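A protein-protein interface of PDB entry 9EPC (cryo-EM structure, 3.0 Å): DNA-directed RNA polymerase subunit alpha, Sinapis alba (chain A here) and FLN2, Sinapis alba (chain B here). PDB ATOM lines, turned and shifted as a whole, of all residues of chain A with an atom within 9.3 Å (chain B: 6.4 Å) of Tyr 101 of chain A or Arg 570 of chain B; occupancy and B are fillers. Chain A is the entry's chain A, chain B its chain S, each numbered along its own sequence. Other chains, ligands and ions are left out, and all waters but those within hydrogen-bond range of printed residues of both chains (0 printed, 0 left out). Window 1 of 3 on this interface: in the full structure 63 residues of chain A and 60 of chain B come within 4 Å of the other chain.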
ATOM      1  N   GLU A  56       8.113  28.547   8.809  1.00  0.00           N
ATOM      2  CA  GLU A  56       7.407  27.615   9.681  1.00  0.00           C
ATOM      3  C   GLU A  56       8.372  26.750  10.479  1.00  0.00           C
ATOM      4  O   GLU A  56       8.022  25.644  10.895  1.00  0.00           O
ATOM      5  CB  GLU A  56       6.448  26.734   8.882  1.00  0.00           C
ATOM      6  CG  GLU A  56       5.353  27.493   8.158  1.00  0.00           C
ATOM      7  CD  GLU A  56       4.405  28.200   9.106  1.00  0.00           C
ATOM      8  OE1 GLU A  56       4.282  27.760  10.268  1.00  0.00           O
ATOM      9  OE2 GLU A  56       3.784  29.199   8.687  1.00  0.00           O
ATOM     10  N   ILE A  57       9.591  27.232  10.704  1.00  0.00           N
ATOM     11  CA  ILE A  57      10.589  26.510  11.481  1.00  0.00           C
ATOM     12  C   ILE A  57      11.016  27.397  12.638  1.00  0.00           C
ATOM     13  O   ILE A  57      11.514  28.509  12.425  1.00  0.00           O
ATOM     14  CB  ILE A  57      11.798  26.102  10.629  1.00  0.00           C
ATOM     15  CG1 ILE A  57      11.358  25.187   9.490  1.00  0.00           C
ATOM     16  CG2 ILE A  57      12.833  25.403  11.484  1.00  0.00           C
ATOM     17  CD1 ILE A  57      12.503  24.643   8.683  1.00  0.00           C
ATOM     18  N   GLU A  58      10.824  26.908  13.859  1.00  0.00           N
ATOM     19  CA  GLU A  58      11.184  27.678  15.037  1.00  0.00           C
ATOM     20  C   GLU A  58      12.693  27.696  15.232  1.00  0.00           C
ATOM     21  O   GLU A  58      13.399  26.737  14.912  1.00  0.00           O
ATOM     22  CB  GLU A  58      10.515  27.101  16.285  1.00  0.00           C
ATOM     23  CG  GLU A  58       9.017  27.319  16.365  1.00  0.00           C
ATOM     24  CD  GLU A  58       8.239  26.386  15.463  1.00  0.00           C
ATOM     25  OE1 GLU A  58       8.856  25.476  14.871  1.00  0.00           O
ATOM     26  OE2 GLU A  58       7.008  26.560  15.348  1.00  0.00           O
ATOM     27  N   GLY A  59      13.185  28.812  15.766  1.00  0.00           N
ATOM     28  CA  GLY A  59      14.567  28.915  16.167  1.00  0.00           C
ATOM     29  C   GLY A  59      14.664  29.600  17.514  1.00  0.00           C
ATOM     30  O   GLY A  59      13.729  30.254  17.972  1.00  0.00           O
ATOM     31  N   THR A  60      15.818  29.434  18.150  1.00  0.00           N
ATOM     32  CA  THR A  60      16.062  29.984  19.473  1.00  0.00           C
ATOM     33  C   THR A  60      17.247  30.936  19.415  1.00  0.00           C
ATOM     34  O   THR A  60      18.267  30.627  18.792  1.00  0.00           O
ATOM     35  CB  THR A  60      16.319  28.872  20.492  1.00  0.00           C
ATOM     36  OG1 THR A  60      16.420  29.437  21.803  1.00  0.00           O
ATOM     37  CG2 THR A  60      17.597  28.138  20.161  1.00  0.00           C
ATOM     38  N   SER A  98      17.991  24.613  20.229  1.00  0.00           N
ATOM     39  CA  SER A  98      17.221  24.062  21.335  1.00  0.00           C
ATOM     40  C   SER A  98      15.890  23.524  20.836  1.00  0.00           C
ATOM     41  O   SER A  98      15.189  24.196  20.074  1.00  0.00           O
ATOM     42  CB  SER A  98      16.985  25.118  22.413  1.00  0.00           C
ATOM     43  OG  SER A  98      16.198  24.593  23.466  1.00  0.00           O
ATOM     44  N   ASN A  99      15.532  22.316  21.259  1.00  0.00           N
ATOM     45  CA  ASN A  99      14.284  21.692  20.848  1.00  0.00           C
ATOM     46  C   ASN A  99      13.123  22.020  21.773  1.00  0.00           C
ATOM     47  O   ASN A  99      11.996  21.595  21.503  1.00  0.00           O
ATOM     48  CB  ASN A  99      14.461  20.176  20.767  1.00  0.00           C
ATOM     49  CG  ASN A  99      15.551  19.771  19.804  1.00  0.00           C
ATOM     50  OD1 ASN A  99      15.710  20.370  18.742  1.00  0.00           O
ATOM     51  ND2 ASN A  99      16.316  18.752  20.173  1.00  0.00           N
ATOM     52  N   LEU A 100      13.363  22.764  22.847  1.00  0.00           N
ATOM     53  CA  LEU A 100      12.345  23.065  23.839  1.00  0.00           C
ATOM     54  C   LEU A 100      11.900  24.516  23.722  1.00  0.00           C
ATOM     55  O   LEU A 100      12.646  25.376  23.250  1.00  0.00           O
ATOM     56  CB  LEU A 100      12.862  22.795  25.252  1.00  0.00           C
ATOM     57  CG  LEU A 100      13.301  21.360  25.530  1.00  0.00           C
ATOM     58  CD1 LEU A 100      13.796  21.221  26.956  1.00  0.00           C
ATOM     59  CD2 LEU A 100      12.160  20.402  25.264  1.00  0.00           C
ATOM     60  N   TYR A 101      10.676  24.780  24.165  1.00  0.00           N
ATOM     61  CA  TYR A 101      10.116  26.119  24.162  1.00  0.00           C
ATOM     62  C   TYR A 101      10.321  26.776  25.523  1.00  0.00           C
ATOM     63  O   TYR A 101      10.905  26.201  26.443  1.00  0.00           O
ATOM     64  CB  TYR A 101       8.632  26.081  23.796  1.00  0.00           C
ATOM     65  CG  TYR A 101       8.351  25.553  22.413  1.00  0.00           C
ATOM     66  CD1 TYR A 101       8.176  24.197  22.192  1.00  0.00           C
ATOM     67  CD2 TYR A 101       8.253  26.411  21.331  1.00  0.00           C
ATOM     68  CE1 TYR A 101       7.917  23.709  20.932  1.00  0.00           C
ATOM     69  CE2 TYR A 101       7.995  25.933  20.066  1.00  0.00           C
ATOM     70  CZ  TYR A 101       7.827  24.581  19.873  1.00  0.00           C
ATOM     71  OH  TYR A 101       7.568  24.098  18.612  1.00  0.00           O
ATOM     72  N   GLY A 102       9.826  28.000  25.648  1.00  0.00           N
ATOM     73  CA  GLY A 102       9.903  28.733  26.893  1.00  0.00           C
ATOM     74  C   GLY A 102      11.104  29.660  26.957  1.00  0.00           C
ATOM     75  O   GLY A 102      12.083  29.518  26.226  1.00  0.00           O
ATOM     76  N   THR A 103      11.013  30.629  27.863  1.00  0.00           N
ATOM     77  CA  THR A 103      12.081  31.594  28.076  1.00  0.00           C
ATOM     78  C   THR A 103      13.051  31.058  29.120  1.00  0.00           C
ATOM     79  O   THR A 103      12.636  30.638  30.204  1.00  0.00           O
ATOM     80  CB  THR A 103      11.511  32.939  28.524  1.00  0.00           C
ATOM     81  OG1 THR A 103      10.603  33.429  27.530  1.00  0.00           O
ATOM     82  CG2 THR A 103      12.628  33.949  28.718  1.00  0.00           C
ATOM     83  N   ARG A 104      14.339  31.074  28.790  1.00  0.00           N
ATOM     84  CA  ARG A 104      15.372  30.523  29.651  1.00  0.00           C
ATOM     85  C   ARG A 104      16.448  31.568  29.894  1.00  0.00           C
ATOM     86  O   ARG A 104      16.662  32.465  29.075  1.00  0.00           O
ATOM     87  CB  ARG A 104      15.992  29.266  29.041  1.00  0.00           C
ATOM     88  CG  ARG A 104      14.980  28.192  28.707  1.00  0.00           C
ATOM     89  CD  ARG A 104      15.586  27.129  27.820  1.00  0.00           C
ATOM     90  NE  ARG A 104      14.638  26.682  26.809  1.00  0.00           N
ATOM     91  CZ  ARG A 104      14.408  27.323  25.672  1.00  0.00           C
ATOM     92  NH1 ARG A 104      15.047  28.440  25.368  1.00  0.00           N
ATOM     93  NH2 ARG A 104      13.513  26.835  24.821  1.00  0.00           N
ATOM     94  N   PRO A 124      21.744  27.092  29.823  1.00  0.00           N
ATOM     95  CA  PRO A 124      20.984  26.015  30.452  1.00  0.00           C
ATOM     96  C   PRO A 124      21.087  24.743  29.633  1.00  0.00           C
ATOM     97  O   PRO A 124      21.418  24.794  28.439  1.00  0.00           O
ATOM     98  CB  PRO A 124      19.549  26.560  30.466  1.00  0.00           C
ATOM     99  CG  PRO A 124      19.511  27.520  29.340  1.00  0.00           C
ATOM    100  CD  PRO A 124      20.868  28.152  29.300  1.00  0.00           C
ATOM    101  N   SER A 126      18.945  22.962  28.259  1.00  0.00           N
ATOM    102  CA  SER A 126      18.022  22.878  27.133  1.00  0.00           C
ATOM    103  C   SER A 126      18.670  23.354  25.840  1.00  0.00           C
ATOM    104  O   SER A 126      18.494  22.736  24.784  1.00  0.00           O
ATOM    105  CB  SER A 126      16.763  23.689  27.429  1.00  0.00           C
ATOM    106  OG  SER A 126      15.928  23.761  26.287  1.00  0.00           O
ATOM    107  N   VAL A 127      19.422  24.447  25.899  1.00  0.00           N
ATOM    108  CA  VAL A 127      19.975  25.068  24.709  1.00  0.00           C
ATOM    109  C   VAL A 127      21.447  24.703  24.584  1.00  0.00           C
ATOM    110  O   VAL A 127      22.122  24.363  25.559  1.00  0.00           O
ATOM    111  CB  VAL A 127      19.787  26.602  24.724  1.00  0.00           C
ATOM    112  CG1 VAL A 127      18.392  26.959  25.201  1.00  0.00           C
ATOM    113  CG2 VAL A 127      20.834  27.257  25.597  1.00  0.00           C
ATOM    114  N   ILE A 151      16.778  33.563  26.749  1.00  0.00           N
ATOM    115  CA  ILE A 151      16.783  32.743  25.545  1.00  0.00           C
ATOM    116  C   ILE A 151      15.370  32.233  25.318  1.00  0.00           C
ATOM    117  O   ILE A 151      14.747  31.689  26.237  1.00  0.00           O
ATOM    118  CB  ILE A 151      17.773  31.573  25.663  1.00  0.00           C
ATOM    119  CG1 ILE A 151      19.126  32.064  26.170  1.00  0.00           C
ATOM    120  CG2 ILE A 151      17.933  30.883  24.329  1.00  0.00           C
ATOM    121  CD1 ILE A 151      19.757  33.103  25.293  1.00  0.00           C
ATOM    122  N   GLU A 152      14.863  32.410  24.102  1.00  0.00           N
ATOM    123  CA  GLU A 152      13.508  31.991  23.783  1.00  0.00           C
ATOM    124  C   GLU A 152      13.471  31.385  22.390  1.00  0.00           C
ATOM    125  O   GLU A 152      14.180  31.836  21.487  1.00  0.00           O
ATOM    126  CB  GLU A 152      12.528  33.165  23.874  1.00  0.00           C
ATOM    127  CG  GLU A 152      11.070  32.769  23.748  1.00  0.00           C
ATOM    128  CD  GLU A 152      10.131  33.920  24.039  1.00  0.00           C
ATOM    129  OE1 GLU A 152      10.622  35.035  24.311  1.00  0.00           O
ATOM    130  OE2 GLU A 152       8.900  33.709  23.999  1.00  0.00           O
ATOM    131  N   ARG A 153      12.646  30.356  22.228  1.00  0.00           N
ATOM    132  CA  ARG A 153      12.405  29.716  20.944  1.00  0.00           C
ATOM    133  C   ARG A 153      11.031  30.134  20.445  1.00  0.00           C
ATOM    134  O   ARG A 153      10.048  30.049  21.187  1.00  0.00           O
ATOM    135  CB  ARG A 153      12.492  28.195  21.072  1.00  0.00           C
ATOM    136  CG  ARG A 153      12.138  27.431  19.813  1.00  0.00           C
ATOM    137  CD  ARG A 153      12.168  25.938  20.075  1.00  0.00           C
ATOM    138  NE  ARG A 153      11.682  25.166  18.939  1.00  0.00           N
ATOM    139  CZ  ARG A 153      12.459  24.653  17.997  1.00  0.00           C
ATOM    140  NH1 ARG A 153      13.772  24.811  18.022  1.00  0.00           N
ATOM    141  NH2 ARG A 153      11.905  23.962  17.006  1.00  0.00           N
ATOM    142  N   ASN A 154      10.962  30.592  19.200  1.00  0.00           N
ATOM    143  CA  ASN A 154       9.729  31.160  18.675  1.00  0.00           C
ATOM    144  C   ASN A 154       9.782  31.122  17.152  1.00  0.00           C
ATOM    145  O   ASN A 154      10.750  30.643  16.556  1.00  0.00           O
ATOM    146  CB  ASN A 154       9.525  32.583  19.200  1.00  0.00           C
ATOM    147  CG  ASN A 154       8.083  33.023  19.146  1.00  0.00           C
ATOM    148  OD1 ASN A 154       7.312  32.555  18.311  1.00  0.00           O
ATOM    149  ND2 ASN A 154       7.707  33.927  20.041  1.00  0.00           N
ATOM    150  N   ARG A 155       8.727  31.632  16.528  1.00  0.00           N
ATOM    151  CA  ARG A 155       8.616  31.714  15.080  1.00  0.00           C
ATOM    152  C   ARG A 155       8.871  33.137  14.603  1.00  0.00           C
ATOM    153  O   ARG A 155       8.780  34.102  15.366  1.00  0.00           O
ATOM    154  CB  ARG A 155       7.231  31.263  14.611  1.00  0.00           C
ATOM    155  CG  ARG A 155       6.904  29.817  14.910  1.00  0.00           C
ATOM    156  CD  ARG A 155       5.457  29.491  14.571  1.00  0.00           C
ATOM    157  NE  ARG A 155       5.171  29.611  13.147  1.00  0.00           N
ATOM    158  CZ  ARG A 155       4.587  30.660  12.586  1.00  0.00           C
ATOM    159  NH1 ARG A 155       4.217  31.708  13.301  1.00  0.00           N
ATOM    160  NH2 ARG A 155       4.371  30.659  11.274  1.00  0.00           N
ATOM    161  N   PHE A 176      14.270  34.684  14.680  1.00  0.00           N
ATOM    162  CA  PHE A 176      14.246  33.272  15.032  1.00  0.00           C
ATOM    163  C   PHE A 176      14.393  32.348  13.835  1.00  0.00           C
ATOM    164  O   PHE A 176      14.692  31.165  14.022  1.00  0.00           O
ATOM    165  CB  PHE A 176      12.949  32.938  15.767  1.00  0.00           C
ATOM    166  CG  PHE A 176      12.754  33.721  17.025  1.00  0.00           C
ATOM    167  CD1 PHE A 176      13.379  33.338  18.195  1.00  0.00           C
ATOM    168  CD2 PHE A 176      11.944  34.837  17.041  1.00  0.00           C
ATOM    169  CE1 PHE A 176      13.204  34.054  19.353  1.00  0.00           C
ATOM    170  CE2 PHE A 176      11.763  35.555  18.198  1.00  0.00           C
ATOM    171  CZ  PHE A 176      12.395  35.164  19.356  1.00  0.00           C
ATOM    172  N   GLU A 217      11.915  18.729   9.507  1.00  0.00           N
ATOM    173  CA  GLU A 217      11.102  19.589  10.358  1.00  0.00           C
ATOM    174  C   GLU A 217      10.036  20.314   9.550  1.00  0.00           C
ATOM    175  O   GLU A 217       8.899  20.472  10.010  1.00  0.00           O
ATOM    176  CB  GLU A 217      11.990  20.587  11.094  1.00  0.00           C
ATOM    177  CG  GLU A 217      11.371  21.145  12.359  1.00  0.00           C
ATOM    178  CD  GLU A 217      11.224  20.094  13.445  1.00  0.00           C
ATOM    179  OE1 GLU A 217      11.956  19.083  13.402  1.00  0.00           O
ATOM    180  OE2 GLU A 217      10.375  20.278  14.341  1.00  0.00           O
ATOM    181  N   ASN A 221       6.162  19.851  10.218  1.00  0.00           N
ATOM    182  CA  ASN A 221       5.354  21.036  10.475  1.00  0.00           C
ATOM    183  C   ASN A 221       4.227  21.162   9.460  1.00  0.00           C
ATOM    184  O   ASN A 221       3.113  21.566   9.807  1.00  0.00           O
ATOM    185  CB  ASN A 221       6.230  22.285  10.461  1.00  0.00           C
ATOM    186  CG  ASN A 221       7.161  22.350  11.648  1.00  0.00           C
ATOM    187  OD1 ASN A 221       7.312  21.377  12.385  1.00  0.00           O
ATOM    188  ND2 ASN A 221       7.798  23.496  11.839  1.00  0.00           N
ATOM    189  N   ASN A 224       1.428  18.749  10.432  1.00  0.00           N
ATOM    190  CA  ASN A 224       0.642  19.280  11.538  1.00  0.00           C
ATOM    191  C   ASN A 224      -0.270  20.418  11.106  1.00  0.00           C
ATOM    192  O   ASN A 224      -1.188  20.776  11.850  1.00  0.00           O
ATOM    193  CB  ASN A 224       1.558  19.756  12.661  1.00  0.00           C
ATOM    194  CG  ASN A 224       2.303  18.622  13.319  1.00  0.00           C
ATOM    195  OD1 ASN A 224       1.866  17.474  13.279  1.00  0.00           O
ATOM    196  ND2 ASN A 224       3.434  18.935  13.934  1.00  0.00           N
ATOM    197  N   TYR B 539      -0.310  14.516  26.111  1.00  0.00           N
ATOM    198  CA  TYR B 539       0.707  13.906  26.947  1.00  0.00           C
ATOM    199  C   TYR B 539       0.316  13.997  28.416  1.00  0.00           C
ATOM    200  O   TYR B 539      -0.363  14.944  28.822  1.00  0.00           O
ATOM    201  CB  TYR B 539       2.066  14.590  26.749  1.00  0.00           C
ATOM    202  CG  TYR B 539       2.639  14.463  25.358  1.00  0.00           C
ATOM    203  CD1 TYR B 539       2.090  15.161  24.294  1.00  0.00           C
ATOM    204  CD2 TYR B 539       3.738  13.657  25.114  1.00  0.00           C
ATOM    205  CE1 TYR B 539       2.612  15.049  23.024  1.00  0.00           C
ATOM    206  CE2 TYR B 539       4.266  13.540  23.848  1.00  0.00           C
ATOM    207  CZ  TYR B 539       3.700  14.239  22.807  1.00  0.00           C
ATOM    208  OH  TYR B 539       4.226  14.125  21.543  1.00  0.00           O
ATOM    209  N   ILE B 567      -1.592  17.287  28.766  1.00  0.00           N
ATOM    210  CA  ILE B 567      -0.999  18.514  28.260  1.00  0.00           C
ATOM    211  C   ILE B 567      -0.774  18.354  26.765  1.00  0.00           C
ATOM    212  O   ILE B 567      -0.638  17.238  26.257  1.00  0.00           O
ATOM    213  CB  ILE B 567       0.322  18.853  28.976  1.00  0.00           C
ATOM    214  CG1 ILE B 567       1.340  17.735  28.766  1.00  0.00           C
ATOM    215  CG2 ILE B 567       0.083  19.068  30.457  1.00  0.00           C
ATOM    216  CD1 ILE B 567       2.661  17.982  29.446  1.00  0.00           C
ATOM    217  N   THR B 568      -0.740  19.477  26.057  1.00  0.00           N
ATOM    218  CA  THR B 568      -0.516  19.425  24.624  1.00  0.00           C
ATOM    219  C   THR B 568       0.963  19.193  24.326  1.00  0.00           C
ATOM    220  O   THR B 568       1.811  19.159  25.221  1.00  0.00           O
ATOM    221  CB  THR B 568      -0.991  20.711  23.950  1.00  0.00           C
ATOM    222  OG1 THR B 568      -0.256  21.825  24.469  1.00  0.00           O
ATOM    223  CG2 THR B 568      -2.472  20.926  24.202  1.00  0.00           C
ATOM    224  N   GLU B 569       1.264  19.023  23.039  1.00  0.00           N
ATOM    225  CA  GLU B 569       2.647  18.821  22.625  1.00  0.00           C
ATOM    226  C   GLU B 569       3.501  20.036  22.960  1.00  0.00           C
ATOM    227  O   GLU B 569       4.658  19.897  23.370  1.00  0.00           O
ATOM    228  CB  GLU B 569       2.703  18.515  21.131  1.00  0.00           C
ATOM    229  CG  GLU B 569       4.098  18.255  20.601  1.00  0.00           C
ATOM    230  CD  GLU B 569       4.116  18.016  19.104  1.00  0.00           C
ATOM    231  OE1 GLU B 569       3.030  18.003  18.488  1.00  0.00           O
ATOM    232  OE2 GLU B 569       5.217  17.844  18.541  1.00  0.00           O
ATOM    233  N   ARG B 570       2.947  21.237  22.786  1.00  0.00           N
ATOM    234  CA  ARG B 570       3.683  22.450  23.124  1.00  0.00           C
ATOM    235  C   ARG B 570       4.012  22.501  24.609  1.00  0.00           C
ATOM    236  O   ARG B 570       5.129  22.865  24.993  1.00  0.00           O
ATOM    237  CB  ARG B 570       2.877  23.681  22.711  1.00  0.00           C
ATOM    238  CG  ARG B 570       3.394  24.983  23.290  1.00  0.00           C
ATOM    239  CD  ARG B 570       4.767  25.322  22.747  1.00  0.00           C
ATOM    240  NE  ARG B 570       4.703  25.802  21.373  1.00  0.00           N
ATOM    241  CZ  ARG B 570       4.665  27.082  21.031  1.00  0.00           C
ATOM    242  NH1 ARG B 570       4.697  28.041  21.942  1.00  0.00           N
ATOM    243  NH2 ARG B 570       4.598  27.409  19.744  1.00  0.00           N
ATOM    244  N   GLU B 571       3.052  22.138  25.461  1.00  0.00           N
ATOM    245  CA  GLU B 571       3.305  22.141  26.897  1.00  0.00           C
ATOM    246  C   GLU B 571       4.302  21.061  27.290  1.00  0.00           C
ATOM    247  O   GLU B 571       5.071  21.247  28.240  1.00  0.00           O
ATOM    248  CB  GLU B 571       1.993  21.960  27.658  1.00  0.00           C
ATOM    249  CG  GLU B 571       0.918  22.954  27.263  1.00  0.00           C
ATOM    250  CD  GLU B 571      -0.393  22.713  27.982  1.00  0.00           C
ATOM    251  OE1 GLU B 571      -0.379  22.050  29.040  1.00  0.00           O
ATOM    252  OE2 GLU B 571      -1.438  23.182  27.487  1.00  0.00           O
ATOM    253  N   TYR B 572       4.304  19.931  26.582  1.00  0.00           N
ATOM    254  CA  TYR B 572       5.270  18.881  26.878  1.00  0.00           C
ATOM    255  C   TYR B 572       6.680  19.284  26.472  1.00  0.00           C
ATOM    256  O   TYR B 572       7.654  18.828  27.078  1.00  0.00           O
ATOM    257  CB  TYR B 572       4.870  17.584  26.177  1.00  0.00           C
ATOM    258  CG  TYR B 572       5.836  16.449  26.416  1.00  0.00           C
ATOM    259  CD1 TYR B 572       5.792  15.712  27.588  1.00  0.00           C
ATOM    260  CD2 TYR B 572       6.793  16.116  25.469  1.00  0.00           C
ATOM    261  CE1 TYR B 572       6.674  14.679  27.812  1.00  0.00           C
ATOM    262  CE2 TYR B 572       7.678  15.085  25.684  1.00  0.00           C
ATOM    263  CZ  TYR B 572       7.613  14.369  26.857  1.00  0.00           C
ATOM    264  OH  TYR B 572       8.494  13.338  27.074  1.00  0.00           O
ATOM    265  N   ARG B 573       6.813  20.122  25.451  1.00  0.00           N
ATOM    266  CA  ARG B 573       8.114  20.591  25.001  1.00  0.00           C
ATOM    267  C   ARG B 573       8.531  21.893  25.666  1.00  0.00           C
ATOM    268  O   ARG B 573       9.608  22.409  25.358  1.00  0.00           O
ATOM    269  CB  ARG B 573       8.113  20.774  23.484  1.00  0.00           C
ATOM    270  CG  ARG B 573       7.871  19.498  22.705  1.00  0.00           C
ATOM    271  CD  ARG B 573       7.638  19.801  21.240  1.00  0.00           C
ATOM    272  NE  ARG B 573       7.348  18.598  20.474  1.00  0.00           N
ATOM    273  CZ  ARG B 573       8.225  17.972  19.702  1.00  0.00           C
ATOM    274  NH1 ARG B 573       9.460  18.422  19.557  1.00  0.00           N
ATOM    275  NH2 ARG B 573       7.851  16.872  19.055  1.00  0.00           N
ATOM    276  N   THR B 574       7.710  22.437  26.557  1.00  0.00           N
ATOM    277  CA  THR B 574       8.074  23.653  27.268  1.00  0.00           C
ATOM    278  C   THR B 574       9.110  23.328  28.333  1.00  0.00           C
ATOM    279  O   THR B 574       8.937  22.390  29.115  1.00  0.00           O
ATOM    280  CB  THR B 574       6.842  24.296  27.900  1.00  0.00           C
ATOM    281  OG1 THR B 574       5.905  24.640  26.874  1.00  0.00           O
ATOM    282  CG2 THR B 574       7.229  25.551  28.658  1.00  0.00           C
ATOM    283  N   SER B 575      10.187  24.103  28.360  1.00  0.00           N
ATOM    284  CA  SER B 575      11.283  23.857  29.280  1.00  0.00           C
ATOM    285  C   SER B 575      11.101  24.648  30.568  1.00  0.00           C
ATOM    286  O   SER B 575      10.429  25.682  30.597  1.00  0.00           O
ATOM    287  CB  SER B 575      12.620  24.224  28.638  1.00  0.00           C
ATOM    288  OG  SER B 575      13.688  24.008  29.540  1.00  0.00           O
ATOM    289  N   LYS B 576      11.704  24.142  31.636  1.00  0.00           N
ATOM    290  CA  LYS B 576      11.720  24.872  32.892  1.00  0.00           C
ATOM    291  C   LYS B 576      12.524  26.160  32.718  1.00  0.00           C
ATOM    292  O   LYS B 576      13.557  26.157  32.040  1.00  0.00           O
ATOM    293  CB  LYS B 576      12.326  24.006  33.998  1.00  0.00           C
ATOM    294  CG  LYS B 576      12.164  24.562  35.400  1.00  0.00           C
ATOM    295  CD  LYS B 576      12.665  23.579  36.443  1.00  0.00           C
ATOM    296  CE  LYS B 576      12.421  24.098  37.849  1.00  0.00           C
ATOM    297  NZ  LYS B 576      12.887  23.136  38.884  1.00  0.00           N
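O of Arg 573 of chain B lies within hydrogen-bond range of N of Tyr 101 of chain A. N of Ser 575 of chain B lies within hydrogen-bond range of O of Tyr 101 of chain A.
The backbone carbonyl oxygen (O) of Gly 102 of chain A sits close to the guanidinium group (NH1) of Arg 104 of chain A, 3.3 Å away. The side-chain carboxylate (OE2) of Glu 569 of chain B lies within salt-bridge range of the guanidinium group (NH2) of Arg 573 of chain B, at 2.9 Å. The guanidinium group of Arg 104 of chain A lies within hydrogen-bond range of the side-chain hydroxyl of Ser 126 of chain A (3.2 Å). O of Arg 104 of chain A is in hydrogen-bond range of N of Ile 151 of chain A (2.6 Å). N of Leu 100 of chain A lies close to OG of Ser 98 of chain A (3.4 Å). The side-chain hydroxyl of Ser 98 of chain A is in hydrogen-bond range of the side-chain hydroxyl of Ser 126 of chain A.
Among the printed residues, pairs that only touch across the chains: Leu 100 of chain A with Arg 573 of chain B (3.2 Å), Leu 100 of chain A with Ser 575 of chain B (3.6 Å), Tyr 101 of chain A with Arg 570 of chain B (3.5 Å), Tyr 101 of chain A with Thr 574 of chain B (3.9 Å), Arg 104 of chain A with Ser 575 of chain B (3.7 Å) and Ser 126 of chain A with Ser 575 of chain B (3.7 Å).
Of chain B, only Arg 570 (3.5 Å), Arg 573 (2.9 Å), Thr 574 (3.9 Å) and Ser 575 (2.9 Å) come within 4 Å of Tyr 101 of chain A. Printed residues of chain B within 4 Å of Arg 104 of chain A: Ser 575. Printed residues of chain B within 4 Å of Ser 126 of chain A: Ser 575 (3.7 Å). Arg 153 of chain A touches none of the printed residues of chain B. Thr 574 of chain B touches just one residue of chain A: Tyr 101. Ser 575 of chain B touches four residues of chain A. The nearest residue of chain B that does not touch Tyr 101 of chain A is Glu 569 of chain B (5.6 Å). The nearest printed residue of chain B that does not touch Arg 104 of chain A is Lys 576 of chain B (4.2 Å).
Of the 11 printed residues of chain B, 4 touch a printed residue of chain A. Printed residues of chain B that touch a printed residue of chain A: Arg 570, Arg 573, Thr 574 and Ser 575. Of the 24 printed residues of chain A, 4 touch a printed residue of chain B. Hydrophobic or aromatic side chains of chain A within 4 Å of the printed part of chain B: Leu 100 and Tyr 101. Among the printed residues, 8 pairs touch across the chains. Among the printed residues, no Asp or Glu carboxylate lies within 4 Å of a Lys or Arg side-chain nitrogen of the other chain.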
